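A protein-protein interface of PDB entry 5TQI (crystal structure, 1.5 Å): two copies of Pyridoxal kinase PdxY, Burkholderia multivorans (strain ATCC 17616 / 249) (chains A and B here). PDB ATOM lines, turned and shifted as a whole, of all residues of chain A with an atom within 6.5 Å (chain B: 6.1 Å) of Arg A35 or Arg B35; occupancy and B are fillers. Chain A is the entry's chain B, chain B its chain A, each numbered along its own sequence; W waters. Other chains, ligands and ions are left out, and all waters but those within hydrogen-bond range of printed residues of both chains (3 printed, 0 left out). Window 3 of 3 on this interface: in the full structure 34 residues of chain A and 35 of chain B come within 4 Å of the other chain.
Among the printed residues, pairs that only touch across the chains: Phe A31 with Phe B31 (3.8 Å), Phe A31 with Gln B34 (3.3 Å), Gln A34 with Phe B31 (3.3 Å), Gln A34 with Ile B274 (3.4 Å), Gly A37 with Ile B274 (3.9 Å), Ile A274 with Gln B34 (3.4 Å) and Ile A274 with Val B38 (3.9 Å).
The backbone carbonyl oxygen of Met B33 lies within hydrogen-bond range of the backbone NH of Val B38. The guanidinium group of Arg B35 lies within hydrogen-bond range of the side-chain amide oxygen of Gln B277, 2.9 Å away. OD1 of Asp B278 lies within salt-bridge range of NH2 of Arg B35. O of Ile B274 lies within hydrogen-bond range of NE2 of Gln B277 (3.2 Å). NE of Arg A35 is in hydrogen-bond range of OE1 of Gln A277 (2.9 Å). The side-chain carboxylate (OD1) of Asp A278 lies within salt-bridge range of the guanidinium group (NH2) of Arg A35 (2.8 Å).
Phe A31 touches its own counterpart, Phe B31. Phe A31 touches Gln B34, and with the chains exchanged Gln A34 touches Phe B31. Gln A34 touches Gln B277, and with the chains exchanged Gln A277 touches Gln B34. Gly A37 touches Ile B274, but with the chains exchanged Ile A274 does not touch Gly B37 (4.2 Å).
Of the 15 printed residues of chain B, 6 touch a printed residue of chain A. Hydrophobic or aromatic side chains of chain A within 4 Å of the printed part of chain B: Phe A31 and Ile A274.
Of chain A, only Arg A35 (3.4 Å) and Gln A277 (3.4 Å) come within 4 Å of Arg B35. Of the printed residues of chain A, Phe B31 touches Phe A31 (3.8 Å) and Gln A34 (3.3 Å). Printed residues of chain B within 4 Å of Gln A277: Gln B34 and Arg B35. Of the printed residues of chain A, Gln B277 touches Gln A34 and Arg A35. Ala A281 touches none of the printed residues of chain B. The nearest printed residue of chain B that does not touch Ile A274 is Gly B37 (4.2 Å).
Water W1 lies within hydrogen-bond range of OD1 of Asp B278 (2.6 Å) and NH1 of Arg A35 (3.3 Å). Water W3 lies within hydrogen-bond range of the side-chain amide oxygen of Gln B34 (2.7 Å) and the side-chain amide oxygen of Gln A34 (2.8 Å). Water W2 lies within hydrogen-bond range of the guanidinium group (NH1) of Arg B35, the side-chain carboxylate (OD1) of Asp A278 and the guanidinium group (NH1) of Arg B282.
NE2 of Gln A277 lies within hydrogen-bond range of O of Gln B34, 2.9 Å away. The side-chain amide oxygen (OE1) of Gln A277 lies within hydrogen-bond range of the guanidinium group (NH1) of Arg B35, at 3.4 Å. The side-chain amide nitrogen of Gln B277 is in hydrogen-bond range of the backbone carbonyl oxygen of Gln A34 (2.9 Å). The side-chain amide oxygen (OE1) of Gln B277 lies within hydrogen-bond range of the guanidinium group (NH1) of Arg A35 (3.4 Å). The guanidinium group (NH2) of Arg A35 sits close to the guanidinium group (NH2) of Arg B35 (3.4 Å).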
ATOM      1  N   VAL A  30      25.930 -10.446  10.913  1.00  0.00           N
ATOM      2  CA  VAL A  30      24.477 -10.571  10.847  1.00  0.00           C
ATOM      3  C   VAL A  30      24.071 -11.850  10.124  1.00  0.00           C
ATOM      4  O   VAL A  30      23.301 -12.665  10.654  1.00  0.00           O
ATOM      5  CB  VAL A  30      23.858  -9.321  10.196  1.00  0.00           C
ATOM      6  CG1 VAL A  30      22.360  -9.528   9.974  1.00  0.00           C
ATOM      7  CG2 VAL A  30      24.107  -8.089  11.063  1.00  0.00           C
ATOM      8  N   PHE A  31      24.566 -12.045   8.894  1.00  0.00           N
ATOM      9  CA  PHE A  31      24.142 -13.225   8.136  1.00  0.00           C
ATOM     10  C   PHE A  31      24.465 -14.534   8.841  1.00  0.00           C
ATOM     11  O   PHE A  31      23.594 -15.421   8.875  1.00  0.00           O
ATOM     12  CB  PHE A  31      24.666 -13.206   6.695  1.00  0.00           C
ATOM     13  CG  PHE A  31      24.418 -14.507   5.967  1.00  0.00           C
ATOM     14  CD1 PHE A  31      23.180 -14.770   5.398  1.00  0.00           C
ATOM     15  CD2 PHE A  31      25.398 -15.488   5.901  1.00  0.00           C
ATOM     16  CE1 PHE A  31      22.926 -15.978   4.759  1.00  0.00           C
ATOM     17  CE2 PHE A  31      25.154 -16.697   5.258  1.00  0.00           C
ATOM     18  CZ  PHE A  31      23.917 -16.943   4.689  1.00  0.00           C
ATOM     19  N   PRO A  32      25.660 -14.749   9.395  1.00  0.00           N
ATOM     20  CA  PRO A  32      25.895 -16.032  10.071  1.00  0.00           C
ATOM     21  C   PRO A  32      24.946 -16.283  11.225  1.00  0.00           C
ATOM     22  O   PRO A  32      24.488 -17.418  11.394  1.00  0.00           O
ATOM     23  CB  PRO A  32      27.363 -15.932  10.504  1.00  0.00           C
ATOM     24  CG  PRO A  32      27.955 -15.025   9.430  1.00  0.00           C
ATOM     25  CD  PRO A  32      26.913 -13.984   9.229  1.00  0.00           C
ATOM     26  N   MET A  33      24.633 -15.262  12.028  1.00  0.00           N
ATOM     27  CA  MET A  33      23.703 -15.475  13.136  1.00  0.00           C
ATOM     28  C   MET A  33      22.310 -15.819  12.621  1.00  0.00           C
ATOM     29  O   MET A  33      21.651 -16.720  13.154  1.00  0.00           O
ATOM     30  CB  MET A  33      23.682 -14.259  14.066  1.00  0.00           C
ATOM     31  CG  MET A  33      25.048 -13.979  14.669  1.00  0.00           C
ATOM     32  SD  MET A  33      25.014 -12.842  16.068  1.00  0.00           S
ATOM     33  CE  MET A  33      24.740 -11.275  15.258  1.00  0.00           C
ATOM     34  N   GLN A  34      21.850 -15.113  11.586  1.00  0.00           N
ATOM     35  CA  GLN A  34      20.566 -15.435  10.975  1.00  0.00           C
ATOM     36  C   GLN A  34      20.566 -16.848  10.414  1.00  0.00           C
ATOM     37  O   GLN A  34      19.585 -17.590  10.571  1.00  0.00           O
ATOM     38  CB  GLN A  34      20.282 -14.449   9.848  1.00  0.00           C
ATOM     39  CG  GLN A  34      20.053 -13.027  10.299  1.00  0.00           C
ATOM     40  CD  GLN A  34      19.977 -12.075   9.130  1.00  0.00           C
ATOM     41  OE1 GLN A  34      20.750 -12.185   8.171  1.00  0.00           O
ATOM     42  NE2 GLN A  34      19.031 -11.146   9.187  1.00  0.00           N
ATOM     43  N   ARG A  35      21.652 -17.231   9.736  1.00  0.00           N
ATOM     44  CA  ARG A  35      21.728 -18.560   9.137  1.00  0.00           C
ATOM     45  C   ARG A  35      21.667 -19.643  10.200  1.00  0.00           C
ATOM     46  O   ARG A  35      21.213 -20.762   9.928  1.00  0.00           O
ATOM     47  CB  ARG A  35      23.009 -18.675   8.301  1.00  0.00           C
ATOM     48  CG  ARG A  35      23.134 -19.944   7.485  1.00  0.00           C
ATOM     49  CD  ARG A  35      22.068 -20.006   6.402  1.00  0.00           C
ATOM     50  NE  ARG A  35      22.217 -21.228   5.615  1.00  0.00           N
ATOM     51  CZ  ARG A  35      21.770 -22.418   5.996  1.00  0.00           C
ATOM     52  NH1 ARG A  35      21.137 -22.548   7.158  1.00  0.00           N
ATOM     53  NH2 ARG A  35      21.968 -23.481   5.219  1.00  0.00           N
ATOM     54  N   LEU A  36      22.132 -19.329  11.411  1.00  0.00           N
ATOM     55  CA  LEU A  36      22.099 -20.232  12.554  1.00  0.00           C
ATOM     56  C   LEU A  36      20.770 -20.189  13.305  1.00  0.00           C
ATOM     57  O   LEU A  36      20.649 -20.810  14.367  1.00  0.00           O
ATOM     58  CB  LEU A  36      23.277 -19.929  13.486  1.00  0.00           C
ATOM     59  CG  LEU A  36      24.642 -20.333  12.928  1.00  0.00           C
ATOM     60  CD1 LEU A  36      25.746 -19.697  13.766  1.00  0.00           C
ATOM     61  CD2 LEU A  36      24.788 -21.860  12.901  1.00  0.00           C
ATOM     62  N   GLY A  37      19.768 -19.478  12.787  1.00  0.00           N
ATOM     63  CA  GLY A  37      18.446 -19.503  13.387  1.00  0.00           C
ATOM     64  C   GLY A  37      18.194 -18.475  14.470  1.00  0.00           C
ATOM     65  O   GLY A  37      17.291 -18.674  15.294  1.00  0.00           O
ATOM     66  N   VAL A  38      18.962 -17.389  14.501  1.00  0.00           N
ATOM     67  CA  VAL A  38      18.790 -16.314  15.472  1.00  0.00           C
ATOM     68  C   VAL A  38      18.433 -15.039  14.720  1.00  0.00           C
ATOM     69  O   VAL A  38      19.079 -14.704  13.723  1.00  0.00           O
ATOM     70  CB  VAL A  38      20.071 -16.120  16.307  1.00  0.00           C
ATOM     71  CG1 VAL A  38      19.952 -14.903  17.218  1.00  0.00           C
ATOM     72  CG2 VAL A  38      20.346 -17.370  17.121  1.00  0.00           C
ATOM     73  N   ARG A 241      21.073 -20.196  20.884  1.00  0.00           N
ATOM     74  CA  ARG A 241      20.375 -21.437  20.563  1.00  0.00           C
ATOM     75  C   ARG A 241      20.390 -22.440  21.709  1.00  0.00           C
ATOM     76  O   ARG A 241      19.768 -23.499  21.577  1.00  0.00           O
ATOM     77  CB  ARG A 241      20.961 -22.089  19.308  1.00  0.00           C
ATOM     78  CG  ARG A 241      20.837 -21.273  18.020  1.00  0.00           C
ATOM     79  CD  ARG A 241      19.379 -21.001  17.607  1.00  0.00           C
ATOM     80  NE  ARG A 241      18.549 -22.200  17.601  1.00  0.00           N
ATOM     81  CZ  ARG A 241      18.376 -22.994  16.547  1.00  0.00           C
ATOM     82  NH1 ARG A 241      18.978 -22.718  15.397  1.00  0.00           N
ATOM     83  NH2 ARG A 241      17.593 -24.064  16.644  1.00  0.00           N
ATOM     84  N   ILE A 274      28.884 -16.298   2.025  1.00  0.00           N
ATOM     85  CA  ILE A 274      27.640 -16.842   1.483  1.00  0.00           C
ATOM     86  C   ILE A 274      27.880 -18.202   0.836  1.00  0.00           C
ATOM     87  O   ILE A 274      27.056 -19.119   0.961  1.00  0.00           O
ATOM     88  CB  ILE A 274      26.989 -15.847   0.502  1.00  0.00           C
ATOM     89  CG1 ILE A 274      26.789 -14.472   1.160  1.00  0.00           C
ATOM     90  CG2 ILE A 274      25.670 -16.412  -0.043  1.00  0.00           C
ATOM     91  CD1 ILE A 274      26.195 -14.503   2.559  1.00  0.00           C
ATOM     92  N   GLN A 277      27.772 -20.989   3.430  1.00  0.00           N
ATOM     93  CA  GLN A 277      26.710 -20.845   4.420  1.00  0.00           C
ATOM     94  C   GLN A 277      26.234 -22.186   4.972  1.00  0.00           C
ATOM     95  O   GLN A 277      25.862 -22.275   6.149  1.00  0.00           O
ATOM     96  CB  GLN A 277      25.542 -20.054   3.850  1.00  0.00           C
ATOM     97  CG  GLN A 277      24.801 -20.749   2.728  1.00  0.00           C
ATOM     98  CD  GLN A 277      23.603 -19.950   2.310  1.00  0.00           C
ATOM     99  OE1 GLN A 277      22.569 -19.973   2.978  1.00  0.00           O
ATOM    100  NE2 GLN A 277      23.738 -19.219   1.210  1.00  0.00           N
ATOM    101  N   ASP A 278      26.207 -23.233   4.144  1.00  0.00           N
ATOM    102  CA  ASP A 278      25.722 -24.516   4.645  1.00  0.00           C
ATOM    103  C   ASP A 278      26.680 -25.100   5.668  1.00  0.00           C
ATOM    104  O   ASP A 278      26.250 -25.820   6.582  1.00  0.00           O
ATOM    105  CB  ASP A 278      25.510 -25.494   3.495  1.00  0.00           C
ATOM    106  CG  ASP A 278      24.290 -25.150   2.643  1.00  0.00           C
ATOM    107  OD1 ASP A 278      23.538 -24.197   2.977  1.00  0.00           O
ATOM    108  OD2 ASP A 278      24.088 -25.848   1.626  1.00  0.00           O
ATOM    109  N   GLU A 279      27.974 -24.805   5.520  1.00  0.00           N
ATOM    110  CA  GLU A 279      28.974 -25.248   6.478  1.00  0.00           C
ATOM    111  C   GLU A 279      28.910 -24.440   7.766  1.00  0.00           C
ATOM    112  O   GLU A 279      29.294 -24.941   8.827  1.00  0.00           O
ATOM    113  CB  GLU A 279      30.364 -25.115   5.860  1.00  0.00           C
ATOM    114  CG  GLU A 279      30.660 -26.129   4.772  1.00  0.00           C
ATOM    115  CD  GLU A 279      31.136 -27.458   5.317  1.00  0.00           C
ATOM    116  OE1 GLU A 279      31.585 -27.504   6.481  1.00  0.00           O
ATOM    117  OE2 GLU A 279      31.056 -28.462   4.582  1.00  0.00           O
ATOM    118  N   ILE A 280      28.475 -23.179   7.699  1.00  0.00           N
ATOM    119  CA  ILE A 280      28.226 -22.437   8.932  1.00  0.00           C
ATOM    120  C   ILE A 280      27.167 -23.153   9.762  1.00  0.00           C
ATOM    121  O   ILE A 280      27.328 -23.354  10.973  1.00  0.00           O
ATOM    122  CB  ILE A 280      27.833 -20.982   8.626  1.00  0.00           C
ATOM    123  CG1 ILE A 280      28.986 -20.241   7.946  1.00  0.00           C
ATOM    124  CG2 ILE A 280      27.393 -20.266   9.909  1.00  0.00           C
ATOM    125  CD1 ILE A 280      28.636 -18.842   7.534  1.00  0.00           C
ATOM    126  N   ALA A 281      26.073 -23.569   9.111  1.00  0.00           N
ATOM    127  CA  ALA A 281      24.991 -24.232   9.829  1.00  0.00           C
ATOM    128  C   ALA A 281      25.373 -25.648  10.247  1.00  0.00           C
ATOM    129  O   ALA A 281      25.017 -26.095  11.345  1.00  0.00           O
ATOM    130  CB  ALA A 281      23.732 -24.263   8.964  1.00  0.00           C
ATOM    131  N   VAL B  30      17.790  -8.625   1.918  1.00  0.00           N
ATOM    132  CA  VAL B  30      19.182  -9.060   1.862  1.00  0.00           C
ATOM    133  C   VAL B  30      19.302 -10.516   2.274  1.00  0.00           C
ATOM    134  O   VAL B  30      19.852 -11.337   1.525  1.00  0.00           O
ATOM    135  CB  VAL B  30      20.081  -8.142   2.709  1.00  0.00           C
ATOM    136  CG1 VAL B  30      21.499  -8.719   2.807  1.00  0.00           C
ATOM    137  CG2 VAL B  30      20.110  -6.742   2.124  1.00  0.00           C
ATOM    138  N   PHE B  31      18.790 -10.860   3.469  1.00  0.00           N
ATOM    139  CA  PHE B  31      18.910 -12.236   3.947  1.00  0.00           C
ATOM    140  C   PHE B  31      18.300 -13.249   2.991  1.00  0.00           C
ATOM    141  O   PHE B  31      18.949 -14.274   2.722  1.00  0.00           O
ATOM    142  CB  PHE B  31      18.389 -12.404   5.382  1.00  0.00           C
ATOM    143  CG  PHE B  31      18.325 -13.838   5.812  1.00  0.00           C
ATOM    144  CD1 PHE B  31      19.470 -14.503   6.226  1.00  0.00           C
ATOM    145  CD2 PHE B  31      17.136 -14.542   5.744  1.00  0.00           C
ATOM    146  CE1 PHE B  31      19.426 -15.848   6.601  1.00  0.00           C
ATOM    147  CE2 PHE B  31      17.090 -15.881   6.129  1.00  0.00           C
ATOM    148  CZ  PHE B  31      18.239 -16.529   6.544  1.00  0.00           C
ATOM    149  N   PRO B  32      17.085 -13.061   2.466  1.00  0.00           N
ATOM    150  CA  PRO B  32      16.554 -14.072   1.543  1.00  0.00           C
ATOM    151  C   PRO B  32      17.426 -14.286   0.324  1.00  0.00           C
ATOM    152  O   PRO B  32      17.626 -15.436  -0.086  1.00  0.00           O
ATOM    153  CB  PRO B  32      15.158 -13.536   1.196  1.00  0.00           C
ATOM    154  CG  PRO B  32      14.774 -12.774   2.434  1.00  0.00           C
ATOM    155  CD  PRO B  32      16.041 -12.101   2.879  1.00  0.00           C
ATOM    156  N   MET B  33      17.954 -13.213  -0.274  1.00  0.00           N
ATOM    157  CA  MET B  33      18.828 -13.393  -1.431  1.00  0.00           C
ATOM    158  C   MET B  33      20.108 -14.129  -1.043  1.00  0.00           C
ATOM    159  O   MET B  33      20.560 -15.020  -1.769  1.00  0.00           O
ATOM    160  CB  MET B  33      19.128 -12.047  -2.098  1.00  0.00           C
ATOM    161  CG  MET B  33      17.850 -11.374  -2.624  1.00  0.00           C
ATOM    162  SD  MET B  33      18.156  -9.952  -3.690  1.00  0.00           S
ATOM    163  CE  MET B  33      18.770  -8.748  -2.501  1.00  0.00           C
ATOM    164  N   GLN B  34      20.703 -13.766   0.097  1.00  0.00           N
ATOM    165  CA  GLN B  34      21.887 -14.473   0.581  1.00  0.00           C
ATOM    166  C   GLN B  34      21.577 -15.940   0.831  1.00  0.00           C
ATOM    167  O   GLN B  34      22.369 -16.823   0.480  1.00  0.00           O
ATOM    168  CB  GLN B  34      22.387 -13.826   1.875  1.00  0.00           C
ATOM    169  CG  GLN B  34      23.045 -12.466   1.680  1.00  0.00           C
ATOM    170  CD  GLN B  34      23.360 -11.790   2.993  1.00  0.00           C
ATOM    171  OE1 GLN B  34      22.574 -11.868   3.939  1.00  0.00           O
ATOM    172  NE2 GLN B  34      24.515 -11.122   3.063  1.00  0.00           N
ATOM    173  N   ARG B  35      20.433 -16.216   1.457  1.00  0.00           N
ATOM    174  CA  ARG B  35      20.052 -17.591   1.752  1.00  0.00           C
ATOM    175  C   ARG B  35      19.865 -18.390   0.467  1.00  0.00           C
ATOM    176  O   ARG B  35      20.026 -19.619   0.461  1.00  0.00           O
ATOM    177  CB  ARG B  35      18.760 -17.577   2.579  1.00  0.00           C
ATOM    178  CG  ARG B  35      18.318 -18.918   3.111  1.00  0.00           C
ATOM    179  CD  ARG B  35      19.331 -19.477   4.109  1.00  0.00           C
ATOM    180  NE  ARG B  35      18.900 -20.774   4.614  1.00  0.00           N
ATOM    181  CZ  ARG B  35      19.128 -21.918   3.976  1.00  0.00           C
ATOM    182  NH1 ARG B  35      19.778 -21.912   2.818  1.00  0.00           N
ATOM    183  NH2 ARG B  35      18.702 -23.062   4.488  1.00  0.00           N
ATOM    184  N   LEU B  36      19.501 -17.713  -0.621  1.00  0.00           N
ATOM    185  CA  LEU B  36      19.335 -18.326  -1.928  1.00  0.00           C
ATOM    186  C   LEU B  36      20.642 -18.402  -2.712  1.00  0.00           C
ATOM    187  O   LEU B  36      20.631 -18.792  -3.885  1.00  0.00           O
ATOM    188  CB  LEU B  36      18.266 -17.567  -2.718  1.00  0.00           C
ATOM    189  CG  LEU B  36      16.825 -17.807  -2.254  1.00  0.00           C
ATOM    190  CD1 LEU B  36      15.909 -16.745  -2.827  1.00  0.00           C
ATOM    191  CD2 LEU B  36      16.362 -19.204  -2.662  1.00  0.00           C
ATOM    192  N   GLY B  37      21.767 -18.051  -2.090  1.00  0.00           N
ATOM    193  CA  GLY B  37      23.060 -18.262  -2.708  1.00  0.00           C
ATOM    194  C   GLY B  37      23.563 -17.145  -3.589  1.00  0.00           C
ATOM    195  O   GLY B  37      24.361 -17.402  -4.501  1.00  0.00           O
ATOM    196  N   VAL B  38      23.113 -15.914  -3.362  1.00  0.00           N
ATOM    197  CA  VAL B  38      23.549 -14.738  -4.107  1.00  0.00           C
ATOM    198  C   VAL B  38      24.216 -13.783  -3.125  1.00  0.00           C
ATOM    199  O   VAL B  38      23.723 -13.593  -2.008  1.00  0.00           O
ATOM    200  CB  VAL B  38      22.326 -14.089  -4.798  1.00  0.00           C
ATOM    201  CG1 VAL B  38      22.683 -12.779  -5.466  1.00  0.00           C
ATOM    202  CG2 VAL B  38      21.758 -15.053  -5.829  1.00  0.00           C
ATOM    203  N   ILE B 274      13.448 -15.421   9.423  1.00  0.00           N
ATOM    204  CA  ILE B 274      14.528 -16.323   9.810  1.00  0.00           C
ATOM    205  C   ILE B 274      13.979 -17.709  10.138  1.00  0.00           C
ATOM    206  O   ILE B 274      14.580 -18.729   9.776  1.00  0.00           O
ATOM    207  CB  ILE B 274      15.353 -15.722  10.964  1.00  0.00           C
ATOM    208  CG1 ILE B 274      16.007 -14.388  10.560  1.00  0.00           C
ATOM    209  CG2 ILE B 274      16.384 -16.721  11.482  1.00  0.00           C
ATOM    210  CD1 ILE B 274      16.357 -14.235   9.107  1.00  0.00           C
ATOM    211  N   GLN B 277      13.457 -19.811   6.970  1.00  0.00           N
ATOM    212  CA  GLN B 277      14.526 -19.673   5.983  1.00  0.00           C
ATOM    213  C   GLN B 277      14.711 -20.920   5.123  1.00  0.00           C
ATOM    214  O   GLN B 277      15.059 -20.805   3.942  1.00  0.00           O
ATOM    215  CB  GLN B 277      15.834 -19.310   6.669  1.00  0.00           C
ATOM    216  CG  GLN B 277      16.391 -20.390   7.564  1.00  0.00           C
ATOM    217  CD  GLN B 277      17.717 -19.987   8.107  1.00  0.00           C
ATOM    218  OE1 GLN B 277      18.736 -20.119   7.433  1.00  0.00           O
ATOM    219  NE2 GLN B 277      17.716 -19.428   9.312  1.00  0.00           N
ATOM    220  N   ASP B 278      14.517 -22.116   5.686  1.00  0.00           N
ATOM    221  CA  ASP B 278      14.701 -23.317   4.873  1.00  0.00           C
ATOM    222  C   ASP B 278      13.642 -23.411   3.784  1.00  0.00           C
ATOM    223  O   ASP B 278      13.903 -23.971   2.708  1.00  0.00           O
ATOM    224  CB  ASP B 278      14.689 -24.571   5.749  1.00  0.00           C
ATOM    225  CG  ASP B 278      15.936 -24.701   6.612  1.00  0.00           C
ATOM    226  OD1 ASP B 278      16.827 -23.827   6.538  1.00  0.00           O
ATOM    227  OD2 ASP B 278      16.026 -25.696   7.365  1.00  0.00           O
ATOM    228  N   ILE B 280      12.330 -20.712   2.352  1.00  0.00           N
ATOM    229  CA  ILE B 280      12.773 -19.773   1.324  1.00  0.00           C
ATOM    230  C   ILE B 280      13.677 -20.486   0.326  1.00  0.00           C
ATOM    231  O   ILE B 280      13.499 -20.383  -0.894  1.00  0.00           O
ATOM    232  CB  ILE B 280      13.476 -18.561   1.963  1.00  0.00           C
ATOM    233  CG1 ILE B 280      12.501 -17.784   2.849  1.00  0.00           C
ATOM    234  CG2 ILE B 280      14.062 -17.653   0.874  1.00  0.00           C
ATOM    235  CD1 ILE B 280      13.153 -16.611   3.596  1.00  0.00           C
ATOM    236  N   ALA B 281      14.656 -21.233   0.839  1.00  0.00           N
ATOM    237  CA  ALA B 281      15.604 -21.923  -0.032  1.00  0.00           C
ATOM    238  C   ALA B 281      14.943 -23.059  -0.805  1.00  0.00           C
ATOM    239  O   ALA B 281      15.228 -23.257  -1.997  1.00  0.00           O
ATOM    240  CB  ALA B 281      16.772 -22.450   0.801  1.00  0.00           C
ATOM    241  N   ARG B 282      14.091 -23.839  -0.139  1.00  0.00           N
ATOM    242  CA  ARG B 282      13.476 -25.023  -0.740  1.00  0.00           C
ATOM    243  C   ARG B 282      12.034 -25.133  -0.262  1.00  0.00           C
ATOM    244  O   ARG B 282      11.745 -25.838   0.714  1.00  0.00           O
ATOM    245  CB  ARG B 282      14.264 -26.292  -0.396  1.00  0.00           C
ATOM    246  CG  ARG B 282      15.703 -26.281  -0.908  1.00  0.00           C
ATOM    247  CD  ARG B 282      16.592 -27.348  -0.272  1.00  0.00           C
ATOM    248  NE  ARG B 282      17.964 -27.221  -0.755  1.00  0.00           N
ATOM    249  CZ  ARG B 282      18.892 -26.450  -0.193  1.00  0.00           C
ATOM    250  NH1 ARG B 282      18.606 -25.739   0.895  1.00  0.00           N
ATOM    251  NH2 ARG B 282      20.111 -26.397  -0.718  1.00  0.00           N
HETATM  252  O   HOH W   1      18.448 -23.953   8.505  1.00  0.00           O
HETATM  253  O   HOH W   2      21.067 -23.898   1.427  1.00  0.00           O
HETATM  254  O   HOH W   3      21.863 -10.578   6.221  1.00  0.00           O
